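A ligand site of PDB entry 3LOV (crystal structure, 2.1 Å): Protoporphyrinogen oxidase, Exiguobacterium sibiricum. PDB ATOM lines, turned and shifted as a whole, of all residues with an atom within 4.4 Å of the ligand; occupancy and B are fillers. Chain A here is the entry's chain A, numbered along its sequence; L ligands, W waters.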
ATOM      1  N   VAL A  10      16.272  26.527  28.404  1.00  0.00           N
ATOM      2  CA  VAL A  10      16.320  25.792  27.170  1.00  0.00           C
ATOM      3  C   VAL A  10      15.203  26.311  26.219  1.00  0.00           C
ATOM      4  O   VAL A  10      14.027  26.219  26.521  1.00  0.00           O
ATOM      5  CB  VAL A  10      16.205  24.251  27.401  1.00  0.00           C
ATOM      6  CG1 VAL A  10      16.370  23.496  26.056  1.00  0.00           C
ATOM      7  CG2 VAL A  10      17.254  23.724  28.418  1.00  0.00           C
ATOM      8  N   GLY A  11      15.618  26.837  25.053  1.00  0.00           N
ATOM      9  CA  GLY A  11      14.738  27.412  24.055  1.00  0.00           C
ATOM     10  C   GLY A  11      14.897  28.920  24.060  1.00  0.00           C
ATOM     11  O   GLY A  11      14.858  29.546  25.119  1.00  0.00           O
ATOM     12  N   GLY A  12      15.140  29.488  22.865  1.00  0.00           N
ATOM     13  CA  GLY A  12      15.326  30.892  22.711  1.00  0.00           C
ATOM     14  C   GLY A  12      14.197  31.644  22.032  1.00  0.00           C
ATOM     15  O   GLY A  12      14.447  32.657  21.320  1.00  0.00           O
ATOM     16  N   GLY A  13      12.963  31.195  22.273  1.00  0.00           N
ATOM     17  CA  GLY A  13      11.804  31.942  21.794  1.00  0.00           C
ATOM     18  C   GLY A  13      11.501  33.052  22.790  1.00  0.00           C
ATOM     19  O   GLY A  13      12.313  33.345  23.659  1.00  0.00           O
ATOM     20  N   ILE A  14      10.312  33.651  22.704  1.00  0.00           N
ATOM     21  CA  ILE A  14       9.930  34.706  23.658  1.00  0.00           C
ATOM     22  C   ILE A  14       9.946  34.189  25.146  1.00  0.00           C
ATOM     23  O   ILE A  14      10.309  34.914  26.070  1.00  0.00           O
ATOM     24  CB  ILE A  14       8.557  35.370  23.298  1.00  0.00           C
ATOM     25  CG1 ILE A  14       8.397  36.701  24.097  1.00  0.00           C
ATOM     26  CG2 ILE A  14       7.365  34.365  23.483  1.00  0.00           C
ATOM     27  CD1 ILE A  14       7.110  37.468  23.853  1.00  0.00           C
ATOM     28  N   THR A  15       9.527  32.960  25.386  1.00  0.00           N
ATOM     29  CA  THR A  15       9.401  32.439  26.730  1.00  0.00           C
ATOM     30  C   THR A  15      10.796  32.328  27.385  1.00  0.00           C
ATOM     31  O   THR A  15      11.001  32.734  28.545  1.00  0.00           O
ATOM     32  CB  THR A  15       8.704  31.065  26.733  1.00  0.00           C
ATOM     33  OG1 THR A  15       7.420  31.220  26.089  1.00  0.00           O
ATOM     34  CG2 THR A  15       8.534  30.574  28.181  1.00  0.00           C
ATOM     35  N   LEU A  35      20.302  27.828  25.926  1.00  0.00           N
ATOM     36  CA  LEU A  35      20.519  26.950  24.767  1.00  0.00           C
ATOM     37  C   LEU A  35      19.375  27.044  23.761  1.00  0.00           C
ATOM     38  O   LEU A  35      18.195  26.735  24.077  1.00  0.00           O
ATOM     39  CB  LEU A  35      20.652  25.505  25.256  1.00  0.00           C
ATOM     40  CG  LEU A  35      21.695  25.183  26.354  1.00  0.00           C
ATOM     41  CD1 LEU A  35      21.690  23.668  26.765  1.00  0.00           C
ATOM     42  CD2 LEU A  35      23.074  25.607  25.891  1.00  0.00           C
ATOM     43  N   GLU A  36      19.698  27.448  22.535  1.00  0.00           N
ATOM     44  CA  GLU A  36      18.746  27.501  21.431  1.00  0.00           C
ATOM     45  C   GLU A  36      19.176  26.519  20.352  1.00  0.00           C
ATOM     46  O   GLU A  36      20.327  26.559  19.959  1.00  0.00           O
ATOM     47  CB  GLU A  36      18.698  28.928  20.859  1.00  0.00           C
ATOM     48  CG  GLU A  36      17.991  29.104  19.518  1.00  0.00           C
ATOM     49  CD  GLU A  36      16.593  28.455  19.421  1.00  0.00           C
ATOM     50  OE1 GLU A  36      15.775  28.636  20.336  1.00  0.00           O
ATOM     51  OE2 GLU A  36      16.304  27.817  18.389  1.00  0.00           O
ATOM     52  N   ALA A  37      18.272  25.663  19.889  1.00  0.00           N
ATOM     53  CA  ALA A  37      18.625  24.633  18.899  1.00  0.00           C
ATOM     54  C   ALA A  37      18.999  25.163  17.520  1.00  0.00           C
ATOM     55  O   ALA A  37      19.790  24.549  16.841  1.00  0.00           O
ATOM     56  CB  ALA A  37      17.502  23.646  18.751  1.00  0.00           C
ATOM     57  N   GLY A  42      14.009  33.828  18.865  1.00  0.00           N
ATOM     58  CA  GLY A  42      12.688  34.302  18.431  1.00  0.00           C
ATOM     59  C   GLY A  42      11.602  33.275  18.332  1.00  0.00           C
ATOM     60  O   GLY A  42      10.396  33.592  18.535  1.00  0.00           O
ATOM     61  N   GLY A  43      11.994  32.036  18.044  1.00  0.00           N
ATOM     62  CA  GLY A  43      11.026  30.967  17.954  1.00  0.00           C
ATOM     63  C   GLY A  43      10.065  31.299  16.843  1.00  0.00           C
ATOM     64  O   GLY A  43      10.468  31.647  15.734  1.00  0.00           O
ATOM     65  N   LYS A  44       8.779  31.243  17.154  1.00  0.00           N
ATOM     66  CA  LYS A  44       7.737  31.582  16.157  1.00  0.00           C
ATOM     67  C   LYS A  44       7.676  33.049  15.713  1.00  0.00           C
ATOM     68  O   LYS A  44       7.036  33.380  14.704  1.00  0.00           O
ATOM     69  CB  LYS A  44       6.384  31.173  16.754  1.00  0.00           C
ATOM     70  CG  LYS A  44       6.213  29.667  16.896  1.00  0.00           C
ATOM     71  CD  LYS A  44       5.075  29.337  17.866  1.00  0.00           C
ATOM     72  CE  LYS A  44       4.750  27.873  18.064  1.00  0.00           C
ATOM     73  NZ  LYS A  44       5.838  26.890  18.111  1.00  0.00           N
ATOM     74  N   PRO A  59       3.126  35.378  14.926  1.00  0.00           N
ATOM     75  CA  PRO A  59       2.206  36.295  15.607  1.00  0.00           C
ATOM     76  C   PRO A  59       2.334  37.735  15.061  1.00  0.00           C
ATOM     77  O   PRO A  59       3.443  38.201  14.792  1.00  0.00           O
ATOM     78  CB  PRO A  59       2.695  36.303  17.066  1.00  0.00           C
ATOM     79  CG  PRO A  59       3.568  35.142  17.232  1.00  0.00           C
ATOM     80  CD  PRO A  59       4.066  34.732  15.845  1.00  0.00           C
ATOM     81  N   ASP A  60       1.229  38.430  14.841  1.00  0.00           N
ATOM     82  CA  ASP A  60       1.365  39.809  14.373  1.00  0.00           C
ATOM     83  C   ASP A  60       1.189  40.829  15.484  1.00  0.00           C
ATOM     84  O   ASP A  60       1.561  41.981  15.319  1.00  0.00           O
ATOM     85  CB  ASP A  60       0.465  40.085  13.141  1.00  0.00           C
ATOM     86  CG  ASP A  60      -1.002  40.287  13.474  1.00  0.00           C
ATOM     87  OD1 ASP A  60      -1.438  39.901  14.574  1.00  0.00           O
ATOM     88  OD2 ASP A  60      -1.713  40.870  12.632  1.00  0.00           O
ATOM     89  N   SER A  61       0.637  40.398  16.611  1.00  0.00           N
ATOM     90  CA  SER A  61       0.236  41.323  17.666  1.00  0.00           C
ATOM     91  C   SER A  61      -0.123  40.558  18.925  1.00  0.00           C
ATOM     92  O   SER A  61       0.004  39.338  18.961  1.00  0.00           O
ATOM     93  CB  SER A  61      -0.962  42.163  17.171  1.00  0.00           C
ATOM     94  OG  SER A  61      -2.080  41.355  16.877  1.00  0.00           O
ATOM     95  N   TYR A  62      -0.550  41.283  19.951  1.00  0.00           N
ATOM     96  CA  TYR A  62      -0.978  40.718  21.226  1.00  0.00           C
ATOM     97  C   TYR A  62      -2.131  41.544  21.785  1.00  0.00           C
ATOM     98  O   TYR A  62      -2.281  42.695  21.439  1.00  0.00           O
ATOM     99  CB  TYR A  62       0.165  40.615  22.229  1.00  0.00           C
ATOM    100  CG  TYR A  62       0.735  41.951  22.744  1.00  0.00           C
ATOM    101  CD1 TYR A  62       1.777  42.607  22.099  1.00  0.00           C
ATOM    102  CD2 TYR A  62       0.199  42.534  23.887  1.00  0.00           C
ATOM    103  CE1 TYR A  62       2.274  43.834  22.573  1.00  0.00           C
ATOM    104  CE2 TYR A  62       0.662  43.733  24.355  1.00  0.00           C
ATOM    105  CZ  TYR A  62       1.686  44.378  23.714  1.00  0.00           C
ATOM    106  OH  TYR A  62       2.087  45.524  24.251  1.00  0.00           O
ATOM    107  N   ILE A 174      -7.752  32.888  13.698  1.00  0.00           N
ATOM    108  CA  ILE A 174      -6.633  32.211  13.024  1.00  0.00           C
ATOM    109  C   ILE A 174      -6.191  30.880  13.711  1.00  0.00           C
ATOM    110  O   ILE A 174      -5.651  29.979  13.045  1.00  0.00           O
ATOM    111  CB  ILE A 174      -5.427  33.154  12.832  1.00  0.00           C
ATOM    112  CG1 ILE A 174      -4.849  33.622  14.176  1.00  0.00           C
ATOM    113  CG2 ILE A 174      -5.822  34.402  11.984  1.00  0.00           C
ATOM    114  CD1 ILE A 174      -3.652  34.555  13.985  1.00  0.00           C
ATOM    115  N   TYR A 175      -6.499  30.718  14.999  1.00  0.00           N
ATOM    116  CA  TYR A 175      -6.111  29.529  15.744  1.00  0.00           C
ATOM    117  C   TYR A 175      -6.957  28.280  15.419  1.00  0.00           C
ATOM    118  O   TYR A 175      -6.504  27.136  15.608  1.00  0.00           O
ATOM    119  CB  TYR A 175      -6.125  29.816  17.248  1.00  0.00           C
ATOM    120  CG  TYR A 175      -5.357  31.067  17.670  1.00  0.00           C
ATOM    121  CD1 TYR A 175      -3.985  31.016  17.946  1.00  0.00           C
ATOM    122  CD2 TYR A 175      -6.016  32.303  17.828  1.00  0.00           C
ATOM    123  CE1 TYR A 175      -3.282  32.154  18.368  1.00  0.00           C
ATOM    124  CE2 TYR A 175      -5.316  33.460  18.224  1.00  0.00           C
ATOM    125  CZ  TYR A 175      -3.950  33.378  18.503  1.00  0.00           C
ATOM    126  OH  TYR A 175      -3.258  34.495  18.922  1.00  0.00           O
ATOM    127  N   THR A 255      22.605  24.975  19.408  1.00  0.00           N
ATOM    128  CA  THR A 255      22.974  24.058  20.466  1.00  0.00           C
ATOM    129  C   THR A 255      21.740  23.403  21.052  1.00  0.00           C
ATOM    130  O   THR A 255      21.293  23.752  22.121  1.00  0.00           O
ATOM    131  CB  THR A 255      23.785  24.745  21.545  1.00  0.00           C
ATOM    132  OG1 THR A 255      24.825  25.504  20.940  1.00  0.00           O
ATOM    133  CG2 THR A 255      24.395  23.713  22.500  1.00  0.00           C
ATOM    134  N   PRO A 256      21.203  22.409  20.345  1.00  0.00           N
ATOM    135  CA  PRO A 256      20.033  21.769  20.906  1.00  0.00           C
ATOM    136  C   PRO A 256      20.373  21.000  22.152  1.00  0.00           C
ATOM    137  O   PRO A 256      21.480  20.479  22.272  1.00  0.00           O
ATOM    138  CB  PRO A 256      19.587  20.818  19.795  1.00  0.00           C
ATOM    139  CG  PRO A 256      20.771  20.630  18.959  1.00  0.00           C
ATOM    140  CD  PRO A 256      21.460  21.954  18.976  1.00  0.00           C
ATOM    141  N   LEU A 257      19.435  20.935  23.090  1.00  0.00           N
ATOM    142  CA  LEU A 257      19.577  20.065  24.264  1.00  0.00           C
ATOM    143  C   LEU A 257      19.129  18.696  23.794  1.00  0.00           C
ATOM    144  O   LEU A 257      18.045  18.573  23.240  1.00  0.00           O
ATOM    145  CB  LEU A 257      18.697  20.534  25.425  1.00  0.00           C
ATOM    146  CG  LEU A 257      18.576  19.570  26.609  1.00  0.00           C
ATOM    147  CD1 LEU A 257      19.948  19.453  27.284  1.00  0.00           C
ATOM    148  CD2 LEU A 257      17.475  19.974  27.630  1.00  0.00           C
ATOM    149  N   THR A 284      11.536  25.412  27.803  1.00  0.00           N
ATOM    150  CA  THR A 284      10.570  26.273  27.120  1.00  0.00           C
ATOM    151  C   THR A 284      10.364  25.781  25.692  1.00  0.00           C
ATOM    152  O   THR A 284       9.762  26.468  24.872  1.00  0.00           O
ATOM    153  CB  THR A 284      10.989  27.784  27.165  1.00  0.00           C
ATOM    154  OG1 THR A 284      12.061  28.064  26.256  1.00  0.00           O
ATOM    155  CG2 THR A 284      11.445  28.185  28.566  1.00  0.00           C
ATOM    156  N   ILE A 285      10.856  24.577  25.439  1.00  0.00           N
ATOM    157  CA  ILE A 285      10.840  23.946  24.135  1.00  0.00           C
ATOM    158  C   ILE A 285       9.504  23.185  23.954  1.00  0.00           C
ATOM    159  O   ILE A 285       8.754  23.052  24.903  1.00  0.00           O
ATOM    160  CB  ILE A 285      11.995  22.964  23.985  1.00  0.00           C
ATOM    161  CG1 ILE A 285      11.840  21.764  24.942  1.00  0.00           C
ATOM    162  CG2 ILE A 285      13.320  23.696  24.160  1.00  0.00           C
ATOM    163  CD1 ILE A 285      12.990  20.719  24.794  1.00  0.00           C
ATOM    164  N   PRO A 286       9.228  22.706  22.741  1.00  0.00           N
ATOM    165  CA  PRO A 286       7.933  22.040  22.553  1.00  0.00           C
ATOM    166  C   PRO A 286       7.757  20.850  23.513  1.00  0.00           C
ATOM    167  O   PRO A 286       8.680  20.053  23.723  1.00  0.00           O
ATOM    168  CB  PRO A 286       8.005  21.549  21.107  1.00  0.00           C
ATOM    169  CG  PRO A 286       8.952  22.513  20.390  1.00  0.00           C
ATOM    170  CD  PRO A 286       9.883  23.047  21.458  1.00  0.00           C
ATOM    171  N   GLN A 289       9.128  17.199  23.248  1.00  0.00           N
ATOM    172  CA  GLN A 289      10.524  17.034  23.575  1.00  0.00           C
ATOM    173  C   GLN A 289      10.713  16.984  25.064  1.00  0.00           C
ATOM    174  O   GLN A 289      11.608  16.309  25.534  1.00  0.00           O
ATOM    175  CB  GLN A 289      11.397  18.122  22.967  1.00  0.00           C
ATOM    176  CG  GLN A 289      11.420  18.182  21.414  1.00  0.00           C
ATOM    177  CD  GLN A 289      12.453  19.161  20.967  1.00  0.00           C
ATOM    178  OE1 GLN A 289      13.585  19.097  21.414  1.00  0.00           O
ATOM    179  NE2 GLN A 289      12.073  20.093  20.109  1.00  0.00           N
ATOM    180  N   THR A 310       0.435  25.350  11.074  1.00  0.00           N
ATOM    181  CA  THR A 310      -0.109  26.484  10.361  1.00  0.00           C
ATOM    182  C   THR A 310       0.961  27.005   9.404  1.00  0.00           C
ATOM    183  O   THR A 310       2.141  27.043   9.761  1.00  0.00           O
ATOM    184  CB  THR A 310      -0.511  27.647  11.343  1.00  0.00           C
ATOM    185  OG1 THR A 310      -1.401  27.157  12.365  1.00  0.00           O
ATOM    186  CG2 THR A 310      -1.191  28.817  10.581  1.00  0.00           C
ATOM    187  N   LEU A 406       4.711  27.156  10.729  1.00  0.00           N
ATOM    188  CA  LEU A 406       4.799  27.003  12.168  1.00  0.00           C
ATOM    189  C   LEU A 406       4.341  25.597  12.524  1.00  0.00           C
ATOM    190  O   LEU A 406       3.134  25.354  12.748  1.00  0.00           O
ATOM    191  CB  LEU A 406       3.952  28.074  12.825  1.00  0.00           C
ATOM    192  CG  LEU A 406       4.417  29.499  12.414  1.00  0.00           C
ATOM    193  CD1 LEU A 406       3.574  30.113  11.237  1.00  0.00           C
ATOM    194  CD2 LEU A 406       4.350  30.355  13.609  1.00  0.00           C
ATOM    195  N   GLY A 409       2.423  24.091  16.105  1.00  0.00           N
ATOM    196  CA  GLY A 409       2.522  25.385  16.787  1.00  0.00           C
ATOM    197  C   GLY A 409       1.395  25.665  17.772  1.00  0.00           C
ATOM    198  O   GLY A 409       1.585  26.409  18.729  1.00  0.00           O
ATOM    199  N   LEU A 410       0.220  25.088  17.525  1.00  0.00           N
ATOM    200  CA  LEU A 410      -0.925  25.391  18.328  1.00  0.00           C
ATOM    201  C   LEU A 410      -1.445  24.188  19.109  1.00  0.00           C
ATOM    202  O   LEU A 410      -1.988  23.270  18.552  1.00  0.00           O
ATOM    203  CB  LEU A 410      -2.028  26.027  17.461  1.00  0.00           C
ATOM    204  CG  LEU A 410      -1.674  27.433  16.944  1.00  0.00           C
ATOM    205  CD1 LEU A 410      -2.600  27.893  15.795  1.00  0.00           C
ATOM    206  CD2 LEU A 410      -1.586  28.469  18.085  1.00  0.00           C
ATOM    207  N   GLY A 439       6.098  28.164  28.787  1.00  0.00           N
ATOM    208  CA  GLY A 439       5.787  28.285  27.385  1.00  0.00           C
ATOM    209  C   GLY A 439       4.349  27.992  27.009  1.00  0.00           C
ATOM    210  O   GLY A 439       3.474  27.832  27.845  1.00  0.00           O
ATOM    211  N   LEU A 440       4.132  27.926  25.702  1.00  0.00           N
ATOM    212  CA  LEU A 440       2.767  27.970  25.172  1.00  0.00           C
ATOM    213  C   LEU A 440       1.926  26.731  25.449  1.00  0.00           C
ATOM    214  O   LEU A 440       0.699  26.782  25.326  1.00  0.00           O
ATOM    215  CB  LEU A 440       2.779  28.279  23.697  1.00  0.00           C
ATOM    216  CG  LEU A 440       2.940  27.179  22.633  1.00  0.00           C
ATOM    217  CD1 LEU A 440       2.410  27.824  21.350  1.00  0.00           C
ATOM    218  CD2 LEU A 440       4.373  26.701  22.458  1.00  0.00           C
ATOM    219  N   VAL A 445      -1.670  30.162  25.290  1.00  0.00           N
ATOM    220  CA  VAL A 445      -0.949  30.145  24.050  1.00  0.00           C
ATOM    221  C   VAL A 445      -0.311  31.465  23.608  1.00  0.00           C
ATOM    222  O   VAL A 445       0.698  31.432  22.905  1.00  0.00           O
ATOM    223  CB  VAL A 445      -1.903  29.601  22.954  1.00  0.00           C
ATOM    224  CG1 VAL A 445      -1.347  29.834  21.573  1.00  0.00           C
ATOM    225  CG2 VAL A 445      -2.146  28.114  23.233  1.00  0.00           C
ATOM    226  N   GLY A 446      -0.841  32.600  24.030  1.00  0.00           N
ATOM    227  CA  GLY A 446      -0.462  33.911  23.476  1.00  0.00           C
ATOM    228  C   GLY A 446       0.840  34.487  24.004  1.00  0.00           C
ATOM    229  O   GLY A 446       1.318  34.088  25.053  1.00  0.00           O
ATOM    230  N   LEU A 447       1.402  35.471  23.294  1.00  0.00           N
ATOM    231  CA  LEU A 447       2.679  36.049  23.669  1.00  0.00           C
ATOM    232  C   LEU A 447       2.717  36.516  25.135  1.00  0.00           C
ATOM    233  O   LEU A 447       3.684  36.190  25.868  1.00  0.00           O
ATOM    234  CB  LEU A 447       3.096  37.160  22.714  1.00  0.00           C
ATOM    235  CG  LEU A 447       3.371  36.696  21.309  1.00  0.00           C
ATOM    236  CD1 LEU A 447       3.348  37.857  20.341  1.00  0.00           C
ATOM    237  CD2 LEU A 447       4.671  35.969  21.198  1.00  0.00           C
ATOM    238  N   PRO A 448       1.656  37.211  25.600  1.00  0.00           N
ATOM    239  CA  PRO A 448       1.606  37.678  26.991  1.00  0.00           C
ATOM    240  C   PRO A 448       1.506  36.576  28.018  1.00  0.00           C
ATOM    241  O   PRO A 448       2.072  36.718  29.114  1.00  0.00           O
ATOM    242  CB  PRO A 448       0.339  38.544  27.034  1.00  0.00           C
ATOM    243  CG  PRO A 448       0.144  38.942  25.610  1.00  0.00           C
ATOM    244  CD  PRO A 448       0.475  37.689  24.864  1.00  0.00           C
ATOM    245  N   CYS A 450       2.770  33.519  27.622  1.00  0.00           N
ATOM    246  CA  CYS A 450       4.114  32.955  27.645  1.00  0.00           C
ATOM    247  C   CYS A 450       5.075  33.821  28.461  1.00  0.00           C
ATOM    248  O   CYS A 450       5.881  33.310  29.260  1.00  0.00           O
ATOM    249  CB  CYS A 450       4.623  32.793  26.218  1.00  0.00           C
ATOM    250  SG  CYS A 450       3.808  31.400  25.365  1.00  0.00           S
HETATM  251  P1  LIG L   1       8.551  28.953  20.448  1.00  0.00           P
HETATM  252  O1  LIG L   1       8.364  30.293  19.817  1.00  0.00           O
HETATM  253  O2  LIG L   1       8.078  27.753  19.714  1.00  0.00           O
HETATM  254  O3  LIG L   1      10.093  28.768  20.779  1.00  0.00           O
HETATM  255  C1  LIG L   1      10.658  27.518  21.096  1.00  0.00           C
HETATM  256  C2  LIG L   1      12.184  27.643  20.942  1.00  0.00           C
HETATM  257  O4  LIG L   1      12.832  26.473  21.437  1.00  0.00           O
HETATM  258  C3  LIG L   1      12.555  27.840  19.483  1.00  0.00           C
HETATM  259  O5  LIG L   1      13.489  28.884  19.321  1.00  0.00           O
HETATM  260  C4  LIG L   1      13.123  26.472  19.142  1.00  0.00           C
HETATM  261  O6  LIG L   1      14.114  26.523  18.174  1.00  0.00           O
HETATM  262  C5  LIG L   1      13.738  26.032  20.463  1.00  0.00           C
HETATM  263  N1  LIG L   1      13.929  24.576  20.613  1.00  0.00           N
HETATM  264  C6  LIG L   1      13.200  23.501  20.169  1.00  0.00           C
HETATM  265  N2  LIG L   1      13.783  22.347  20.573  1.00  0.00           N
HETATM  266  C7  LIG L   1      14.910  22.683  21.270  1.00  0.00           C
HETATM  267  C8  LIG L   1      15.892  21.941  21.943  1.00  0.00           C
HETATM  268  N3  LIG L   1      15.833  20.615  22.005  1.00  0.00           N
HETATM  269  N4  LIG L   1      16.928  22.599  22.584  1.00  0.00           N
HETATM  270  C9  LIG L   1      16.974  23.971  22.603  1.00  0.00           C
HETATM  271  N5  LIG L   1      15.987  24.701  21.963  1.00  0.00           N
HETATM  272  C10 LIG L   1      14.993  24.069  21.300  1.00  0.00           C
HETATM  273  N6  LIG L   1       0.237  34.821  20.038  1.00  0.00           N
HETATM  274  C11 LIG L   1      -0.208  36.100  20.190  1.00  0.00           C
HETATM  275  O7  LIG L   1      -0.181  36.649  21.305  1.00  0.00           O
HETATM  276  N7  LIG L   1      -0.717  36.777  19.110  1.00  0.00           N
HETATM  277  C12 LIG L   1      -0.815  36.218  17.885  1.00  0.00           C
HETATM  278  O8  LIG L   1      -1.237  36.885  16.969  1.00  0.00           O
HETATM  279  C13 LIG L   1      -0.402  34.919  17.704  1.00  0.00           C
HETATM  280  N8  LIG L   1      -0.459  34.349  16.444  1.00  0.00           N
HETATM  281  C14 LIG L   1      -0.012  33.029  16.286  1.00  0.00           C
HETATM  282  C15 LIG L   1      -0.085  32.416  15.029  1.00  0.00           C
HETATM  283  C16 LIG L   1       0.345  31.102  14.858  1.00  0.00           C
HETATM  284  C17 LIG L   1       0.275  30.450  13.502  1.00  0.00           C
HETATM  285  C18 LIG L   1       0.901  30.390  15.938  1.00  0.00           C
HETATM  286  C19 LIG L   1       1.380  28.945  15.799  1.00  0.00           C
HETATM  287  C20 LIG L   1       0.995  30.983  17.189  1.00  0.00           C
HETATM  288  C21 LIG L   1       0.540  32.313  17.379  1.00  0.00           C
HETATM  289  N9  LIG L   1       0.635  32.915  18.633  1.00  0.00           N
HETATM  290  C22 LIG L   1       0.147  34.225  18.795  1.00  0.00           C
HETATM  291  C23 LIG L   1       1.180  32.214  19.863  1.00  0.00           C
HETATM  292  C24 LIG L   1       2.678  32.611  20.027  1.00  0.00           C
HETATM  293  O9  LIG L   1       3.365  32.152  18.929  1.00  0.00           O
HETATM  294  C25 LIG L   1       3.315  32.030  21.293  1.00  0.00           C
HETATM  295  O10 LIG L   1       2.791  32.782  22.378  1.00  0.00           O
HETATM  296  C26 LIG L   1       4.862  32.133  21.379  1.00  0.00           C
HETATM  297  O11 LIG L   1       5.542  32.232  20.145  1.00  0.00           O
HETATM  298  C27 LIG L   1       5.464  30.913  22.054  1.00  0.00           C
HETATM  299  O12 LIG L   1       6.833  31.130  22.235  1.00  0.00           O
HETATM  300  P2  LIG L   1       7.688  30.038  22.989  1.00  0.00           P
HETATM  301  O13 LIG L   1       6.940  29.404  24.123  1.00  0.00           O
HETATM  302  O14 LIG L   1       9.093  30.484  23.299  1.00  0.00           O
HETATM  303  O15 LIG L   1       7.827  28.841  21.876  1.00  0.00           O
HETATM  304  O   HOH W   1      -2.187  37.900  22.513  1.00  0.00           O
HETATM  305  O   HOH W   2       7.063  26.655  24.247  1.00  0.00           O
HETATM  306  O   HOH W   3       9.821  26.749  17.881  1.00  0.00           O
HETATM  307  O   HOH W   4      -1.039  36.233  14.248  1.00  0.00           O
HETATM  308  O   HOH W   5       7.544  25.608  21.601  1.00  0.00           O
HETATM  309  O   HOH W   6      11.522  29.793  24.191  1.00  0.00           O
HETATM  310  O   HOH W   7      14.329  30.478  17.381  1.00  0.00           O
HETATM  311  O   HOH W   8       8.538  32.937  20.331  1.00  0.00           O
HETATM  312  O   HOH W   9      -3.051  38.949  17.830  1.00  0.00           O
HETATM  313  O   HOH W  10       0.336  25.892  14.482  1.00  0.00           O
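O5 of the ligand sits at hydrogen-bond distance from OE1 of Glu 36, 2.5 Å away. O10 of the ligand is in hydrogen-bond range of O of Val 445 (2.5 Å). O of Ser 61 sits at hydrogen-bond distance from N7 of the ligand. The backbone NH (N) of Thr 15 lies within hydrogen-bond range of an oxygen (O14) of the ligand, 3.3 Å away. The side-chain hydroxyl (OG1) of Thr 15 is in hydrogen-bond range of an oxygen (O13) of the ligand (2.7 Å). N3 of the ligand is in hydrogen-bond range of OE1 of Gln 289 (2.8 Å). The backbone NH (N) of Leu 447 lies within hydrogen-bond range of an oxygen (O7) of the ligand (2.8 Å). The backbone NH (N) of Lys 44 sits at hydrogen-bond distance from an oxygen (O1) of the ligand (2.9 Å). O2 of the ligand is in salt-bridge range of NZ of Lys 44, 2.9 Å away. N4 of the ligand sits at hydrogen-bond distance from N of Leu 257 (3.1 Å). O of Leu 257 is in hydrogen-bond range of N3 of the ligand (3.3 Å). O of Gly 446 lies close to O10 of the ligand (3.3 Å). OH of Tyr 175 lies close to N7 of the ligand (3.4 Å). The backbone NH of Ala 37 lies within hydrogen-bond range of a nitrogen (N5) of the ligand (3.2 Å). The side-chain sulfur of Cys 450 lies within hydrogen-bond range of an oxygen (O10) of the ligand (3.4 Å). The backbone NH (N) of Ile 14 sits at hydrogen-bond distance from an oxygen (O14) of the ligand (3.4 Å).
OE1 of Glu 36 is in hydrogen-bond range of N of Gly 12 (2.7 Å). The backbone carbonyl oxygen (O) of Glu 36 is in hydrogen-bond range of the backbone NH (N) of Thr 255 (2.8 Å). SG of Cys 450 sits close to OG1 of Thr 15. The backbone NH (N) of Gly 11 lies within hydrogen-bond range of the backbone carbonyl oxygen (O) of Leu 35. The side-chain sulfur (SG) of Cys 450 lies within hydrogen-bond range of the backbone NH (N) of Leu 440 (3.5 Å). O of Val 10 sits at hydrogen-bond distance from OG1 of Thr 284, 2.7 Å away. O of Thr 310 lies within hydrogen-bond range of N of Leu 406, at 2.7 Å. O of Gly 12 lies within hydrogen-bond range of N of Gly 42 (2.8 Å).
Merely in contact with the ligand: Val 10, Gly 11, Gly 12, Gly 13, Leu 35, Gly 43, Pro 59, Asp 60, Pro 256, Ile 285, Pro 286, Thr 310, Leu 406, Gly 409, Leu 410, Gly 439, Leu 440 and Pro 448. Hydrophobic or aromatic side chains that line the ligand: Val 10, Ile 14, Ala 37, Pro 59, Tyr 175, Leu 257, Ile 285, Pro 286, Leu 406, Leu 410, Val 445, Leu 447 and Pro 448. The nearest printed residue that does not touch the ligand is Thr 284 (4.02 Å).
Water W7 lies within hydrogen-bond range of an oxygen (O5) of the ligand (2.6 Å), the backbone NH (N) of Gly 43 (2.9 Å) and the side-chain carboxylate (OE2) of Glu 36 (3.5 Å). Water W6 lies within hydrogen-bond range of an oxygen (O14) of the ligand (2.7 Å), the side-chain hydroxyl (OG1) of Thr 284 (2.7 Å), the backbone NH (N) of Gly 13 (2.8 Å) and the backbone carbonyl oxygen (O) of Gly 11 (3.5 Å). Water W8 lies within hydrogen-bond range of O of Gly 42 (2.7 Å), O1 of the ligand (2.7 Å) and N of Ile 14 (3.0 Å). Water W4 lies within hydrogen-bond range of O8 of the ligand and N of Asp 60. Water W9 lies within hydrogen-bond range of OG of Ser 61 (2.8 Å) and O8 of the ligand (2.9 Å). Water W10 lies within hydrogen-bond range of the side-chain hydroxyl (OG1) of Thr 310 (3.0 Å), the backbone NH (N) of Leu 410 (3.1 Å), the backbone NH (N) of Gly 409 (3.2 Å) and the backbone carbonyl oxygen (O) of Leu 406 (3.3 Å).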
